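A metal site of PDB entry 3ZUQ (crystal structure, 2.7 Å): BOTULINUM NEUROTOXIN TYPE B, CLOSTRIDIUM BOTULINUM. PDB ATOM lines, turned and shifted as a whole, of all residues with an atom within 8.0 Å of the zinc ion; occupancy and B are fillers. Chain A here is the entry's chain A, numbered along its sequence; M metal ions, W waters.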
ATOM      1  N   ASN A 170       9.012  -1.111   1.171  1.00  0.00           N
ATOM      2  CA  ASN A 170       8.903  -0.848   2.601  1.00  0.00           C
ATOM      3  C   ASN A 170       8.147   0.444   2.841  1.00  0.00           C
ATOM      4  O   ASN A 170       8.487   1.477   2.274  1.00  0.00           O
ATOM      5  CB  ASN A 170      10.281  -0.795   3.248  1.00  0.00           C
ATOM      6  CG  ASN A 170      11.107  -2.039   2.960  1.00  0.00           C
ATOM      7  OD1 ASN A 170      10.705  -3.156   3.281  1.00  0.00           O
ATOM      8  ND2 ASN A 170      12.257  -1.846   2.337  1.00  0.00           N
ATOM      9  N   GLU A 171       7.114   0.369   3.677  1.00  0.00           N
ATOM     10  CA  GLU A 171       6.268   1.517   3.945  1.00  0.00           C
ATOM     11  C   GLU A 171       5.910   1.614   5.431  1.00  0.00           C
ATOM     12  O   GLU A 171       5.749   0.592   6.111  1.00  0.00           O
ATOM     13  CB  GLU A 171       4.995   1.461   3.103  1.00  0.00           C
ATOM     14  CG  GLU A 171       4.381   2.830   2.811  1.00  0.00           C
ATOM     15  CD  GLU A 171       2.910   2.761   2.447  1.00  0.00           C
ATOM     16  OE1 GLU A 171       2.500   1.786   1.778  1.00  0.00           O
ATOM     17  OE2 GLU A 171       2.156   3.686   2.841  1.00  0.00           O
ATOM     18  N   THR A 172       5.790   2.845   5.914  1.00  0.00           N
ATOM     19  CA  THR A 172       5.314   3.109   7.266  1.00  0.00           C
ATOM     20  C   THR A 172       3.926   3.728   7.169  1.00  0.00           C
ATOM     21  O   THR A 172       3.725   4.693   6.433  1.00  0.00           O
ATOM     22  CB  THR A 172       6.275   4.050   8.032  1.00  0.00           C
ATOM     23  OG1 THR A 172       7.598   3.525   7.989  1.00  0.00           O
ATOM     24  CG2 THR A 172       5.851   4.210   9.481  1.00  0.00           C
ATOM     25  N   ILE A 227      17.765   0.987   5.471  1.00  0.00           N
ATOM     26  CA  ILE A 227      16.404   1.030   4.948  1.00  0.00           C
ATOM     27  C   ILE A 227      15.413   1.028   6.100  1.00  0.00           C
ATOM     28  O   ILE A 227      14.504   1.871   6.141  1.00  0.00           O
ATOM     29  CB  ILE A 227      16.116  -0.164   3.997  1.00  0.00           C
ATOM     30  CG1 ILE A 227      17.002  -0.068   2.751  1.00  0.00           C
ATOM     31  CG2 ILE A 227      14.645  -0.198   3.613  1.00  0.00           C
ATOM     32  CD1 ILE A 227      16.838  -1.243   1.785  1.00  0.00           C
ATOM     33  N   HIS A 230      15.403   4.338   7.778  1.00  0.00           N
ATOM     34  CA  HIS A 230      14.651   5.316   6.993  1.00  0.00           C
ATOM     35  C   HIS A 230      13.185   5.285   7.405  1.00  0.00           C
ATOM     36  O   HIS A 230      12.541   6.333   7.545  1.00  0.00           O
ATOM     37  CB  HIS A 230      14.805   5.067   5.498  1.00  0.00           C
ATOM     38  CG  HIS A 230      13.960   5.955   4.636  1.00  0.00           C
ATOM     39  ND1 HIS A 230      14.418   7.159   4.132  1.00  0.00           N
ATOM     40  CD2 HIS A 230      12.683   5.827   4.201  1.00  0.00           C
ATOM     41  CE1 HIS A 230      13.457   7.729   3.423  1.00  0.00           C
ATOM     42  NE2 HIS A 230      12.397   6.939   3.447  1.00  0.00           N
ATOM     43  N   GLU A 231      12.664   4.072   7.609  1.00  0.00           N
ATOM     44  CA  GLU A 231      11.284   3.875   8.028  1.00  0.00           C
ATOM     45  C   GLU A 231      11.098   4.218   9.509  1.00  0.00           C
ATOM     46  O   GLU A 231      10.003   4.620   9.912  1.00  0.00           O
ATOM     47  CB  GLU A 231      10.824   2.429   7.780  1.00  0.00           C
ATOM     48  CG  GLU A 231      10.945   1.935   6.342  1.00  0.00           C
ATOM     49  CD  GLU A 231      10.292   2.847   5.318  1.00  0.00           C
ATOM     50  OE1 GLU A 231       9.208   3.406   5.609  1.00  0.00           O
ATOM     51  OE2 GLU A 231      10.861   3.004   4.208  1.00  0.00           O
ATOM     52  N   ILE A 233      12.580   6.688  11.028  1.00  0.00           N
ATOM     53  CA  ILE A 233      12.454   8.137  11.061  1.00  0.00           C
ATOM     54  C   ILE A 233      11.008   8.545  10.781  1.00  0.00           C
ATOM     55  O   ILE A 233      10.486   9.476  11.417  1.00  0.00           O
ATOM     56  CB  ILE A 233      13.413   8.833  10.068  1.00  0.00           C
ATOM     57  CG1 ILE A 233      14.864   8.605  10.480  1.00  0.00           C
ATOM     58  CG2 ILE A 233      13.131  10.329   9.981  1.00  0.00           C
ATOM     59  CD1 ILE A 233      15.886   8.990   9.411  1.00  0.00           C
ATOM     60  N   HIS A 234      10.354   7.866   9.837  1.00  0.00           N
ATOM     61  CA  HIS A 234       8.920   8.048   9.632  1.00  0.00           C
ATOM     62  C   HIS A 234       8.145   7.724  10.909  1.00  0.00           C
ATOM     63  O   HIS A 234       7.334   8.524  11.365  1.00  0.00           O
ATOM     64  CB  HIS A 234       8.405   7.207   8.468  1.00  0.00           C
ATOM     65  CG  HIS A 234       8.848   7.689   7.123  1.00  0.00           C
ATOM     66  ND1 HIS A 234       8.670   8.992   6.698  1.00  0.00           N
ATOM     67  CD2 HIS A 234       9.424   7.036   6.091  1.00  0.00           C
ATOM     68  CE1 HIS A 234       9.131   9.123   5.470  1.00  0.00           C
ATOM     69  NE2 HIS A 234       9.595   7.957   5.078  1.00  0.00           N
ATOM     70  N   LYS A 243       4.229  14.420  11.639  1.00  0.00           N
ATOM     71  CA  LYS A 243       4.306  13.912  10.267  1.00  0.00           C
ATOM     72  C   LYS A 243       3.264  14.617   9.387  1.00  0.00           C
ATOM     73  O   LYS A 243       2.420  13.968   8.751  1.00  0.00           O
ATOM     74  CB  LYS A 243       4.092  12.392  10.275  1.00  0.00           C
ATOM     75  CG  LYS A 243       4.614  11.664   9.051  1.00  0.00           C
ATOM     76  CD  LYS A 243       4.369  10.162   9.159  1.00  0.00           C
ATOM     77  CE  LYS A 243       4.342   9.520   7.783  1.00  0.00           C
ATOM     78  NZ  LYS A 243       3.623   8.217   7.821  1.00  0.00           N
ATOM     79  N   GLU A 267       7.934  15.907   4.297  1.00  0.00           N
ATOM     80  CA  GLU A 267       8.303  14.966   5.352  1.00  0.00           C
ATOM     81  C   GLU A 267       9.239  13.885   4.813  1.00  0.00           C
ATOM     82  O   GLU A 267      10.188  13.494   5.479  1.00  0.00           O
ATOM     83  CB  GLU A 267       7.047  14.341   5.950  1.00  0.00           C
ATOM     84  CG  GLU A 267       7.262  13.618   7.279  1.00  0.00           C
ATOM     85  CD  GLU A 267       7.618  12.146   7.117  1.00  0.00           C
ATOM     86  OE1 GLU A 267       7.525  11.613   5.991  1.00  0.00           O
ATOM     87  OE2 GLU A 267       8.006  11.521   8.136  1.00  0.00           O
ATOM     88  N   GLU A 268       8.955  13.435   3.585  1.00  0.00           N
ATOM     89  CA  GLU A 268       9.767  12.459   2.869  1.00  0.00           C
ATOM     90  C   GLU A 268      11.161  13.003   2.519  1.00  0.00           C
ATOM     91  O   GLU A 268      12.152  12.267   2.583  1.00  0.00           O
ATOM     92  CB  GLU A 268       9.038  12.019   1.598  1.00  0.00           C
ATOM     93  CG  GLU A 268       9.685  10.848   0.883  1.00  0.00           C
ATOM     94  CD  GLU A 268       9.765   9.612   1.747  1.00  0.00           C
ATOM     95  OE1 GLU A 268       8.730   9.257   2.373  1.00  0.00           O
ATOM     96  OE2 GLU A 268      10.842   8.992   1.815  1.00  0.00           O
ATOM     97  N   LEU A 269      11.231  14.277   2.130  1.00  0.00           N
ATOM     98  CA  LEU A 269      12.485  14.893   1.731  1.00  0.00           C
ATOM     99  C   LEU A 269      13.342  15.290   2.927  1.00  0.00           C
ATOM    100  O   LEU A 269      14.563  15.219   2.862  1.00  0.00           O
ATOM    101  CB  LEU A 269      12.239  16.092   0.818  1.00  0.00           C
ATOM    102  CG  LEU A 269      11.722  15.812  -0.593  1.00  0.00           C
ATOM    103  CD1 LEU A 269      11.612  17.102  -1.378  1.00  0.00           C
ATOM    104  CD2 LEU A 269      12.610  14.817  -1.345  1.00  0.00           C
ATOM    105  N   THR A 271      13.279  13.563   5.680  1.00  0.00           N
ATOM    106  CA  THR A 271      13.733  12.233   6.099  1.00  0.00           C
ATOM    107  C   THR A 271      15.003  11.811   5.355  1.00  0.00           C
ATOM    108  O   THR A 271      15.948  11.325   5.976  1.00  0.00           O
ATOM    109  CB  THR A 271      12.623  11.170   5.930  1.00  0.00           C
ATOM    110  OG1 THR A 271      11.497  11.518   6.736  1.00  0.00           O
ATOM    111  CG2 THR A 271      13.120   9.790   6.349  1.00  0.00           C
ATOM    112  N   PHE A 272      15.024  12.001   4.043  1.00  0.00           N
ATOM    113  CA  PHE A 272      16.205  11.673   3.238  1.00  0.00           C
ATOM    114  C   PHE A 272      17.379  12.600   3.544  1.00  0.00           C
ATOM    115  O   PHE A 272      18.523  12.139   3.630  1.00  0.00           O
ATOM    116  CB  PHE A 272      15.896  11.710   1.743  1.00  0.00           C
ATOM    117  CG  PHE A 272      16.968  11.078   0.907  1.00  0.00           C
ATOM    118  CD1 PHE A 272      18.075  11.811   0.495  1.00  0.00           C
ATOM    119  CD2 PHE A 272      16.882   9.728   0.558  1.00  0.00           C
ATOM    120  CE1 PHE A 272      19.086  11.217  -0.259  1.00  0.00           C
ATOM    121  CE2 PHE A 272      17.883   9.127  -0.202  1.00  0.00           C
ATOM    122  CZ  PHE A 272      18.979   9.872  -0.609  1.00  0.00           C
ATOM    123  N   GLU A 358      18.332  10.117   6.791  1.00  0.00           N
ATOM    124  CA  GLU A 358      18.972   9.012   6.065  1.00  0.00           C
ATOM    125  C   GLU A 358      20.424   9.333   5.676  1.00  0.00           C
ATOM    126  O   GLU A 358      21.303   8.472   5.756  1.00  0.00           O
ATOM    127  CB  GLU A 358      18.150   8.616   4.832  1.00  0.00           C
ATOM    128  CG  GLU A 358      18.644   7.327   4.143  1.00  0.00           C
ATOM    129  CD  GLU A 358      17.911   6.998   2.841  1.00  0.00           C
ATOM    130  OE1 GLU A 358      16.679   7.161   2.774  1.00  0.00           O
ATOM    131  OE2 GLU A 358      18.583   6.549   1.884  1.00  0.00           O
ATOM    132  N   ARG A 370      22.111   6.288  -1.867  1.00  0.00           N
ATOM    133  CA  ARG A 370      21.910   7.117  -3.061  1.00  0.00           C
ATOM    134  C   ARG A 370      22.124   8.606  -2.764  1.00  0.00           C
ATOM    135  O   ARG A 370      21.954   9.058  -1.632  1.00  0.00           O
ATOM    136  CB  ARG A 370      20.531   6.870  -3.675  1.00  0.00           C
ATOM    137  CG  ARG A 370      19.396   6.857  -2.674  1.00  0.00           C
ATOM    138  CD  ARG A 370      18.062   6.665  -3.351  1.00  0.00           C
ATOM    139  NE  ARG A 370      16.975   6.719  -2.374  1.00  0.00           N
ATOM    140  CZ  ARG A 370      15.697   6.866  -2.673  1.00  0.00           C
ATOM    141  NH1 ARG A 370      15.315   6.979  -3.947  1.00  0.00           N
ATOM    142  NH2 ARG A 370      14.783   6.906  -1.706  1.00  0.00           N
ATOM    143  N   TYR A 373      16.926  11.727  -3.255  1.00  0.00           N
ATOM    144  CA  TYR A 373      15.657  11.024  -3.381  1.00  0.00           C
ATOM    145  C   TYR A 373      15.298  10.871  -4.861  1.00  0.00           C
ATOM    146  O   TYR A 373      14.533   9.985  -5.239  1.00  0.00           O
ATOM    147  CB  TYR A 373      14.528  11.769  -2.632  1.00  0.00           C
ATOM    148  CG  TYR A 373      13.153  11.171  -2.806  1.00  0.00           C
ATOM    149  CD1 TYR A 373      12.789  10.006  -2.133  1.00  0.00           C
ATOM    150  CD2 TYR A 373      12.224  11.753  -3.659  1.00  0.00           C
ATOM    151  CE1 TYR A 373      11.524   9.447  -2.306  1.00  0.00           C
ATOM    152  CE2 TYR A 373      10.961  11.203  -3.830  1.00  0.00           C
ATOM    153  CZ  TYR A 373      10.621  10.043  -3.154  1.00  0.00           C
ATOM    154  OH  TYR A 373       9.368   9.500  -3.318  1.00  0.00           O
HETATM  155 ZN    ZN M   1      10.291   7.367   3.202  1.00  0.00          ZN
HETATM  156  O   HOH W   1      10.057   5.052   1.095  1.00  0.00           O
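A ring nitrogen (ND1) of His 234 is in hydrogen-bond range of the side-chain carboxylate (OE1) of Glu 267 (2.9 Å).
A ring nitrogen (ND1) of His 230 sits at hydrogen-bond distance from the side-chain carboxylate (OE1) of Glu 358.
Along chain A the residues within 4 Å of the zinc ion span positions 230 to 268.
The nearest printed residue that does not touch the zinc ion is Glu 231 (4.5 Å).
The zinc ion is bound by NE2 of His 234 (2.1 Å), NE2 of His 230 (2.2 Å), OE2 of Glu 268 (2.2 Å) and OE1 of Glu 268 (2.6 Å).
The zinc ion has four donor atoms within binding distance.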
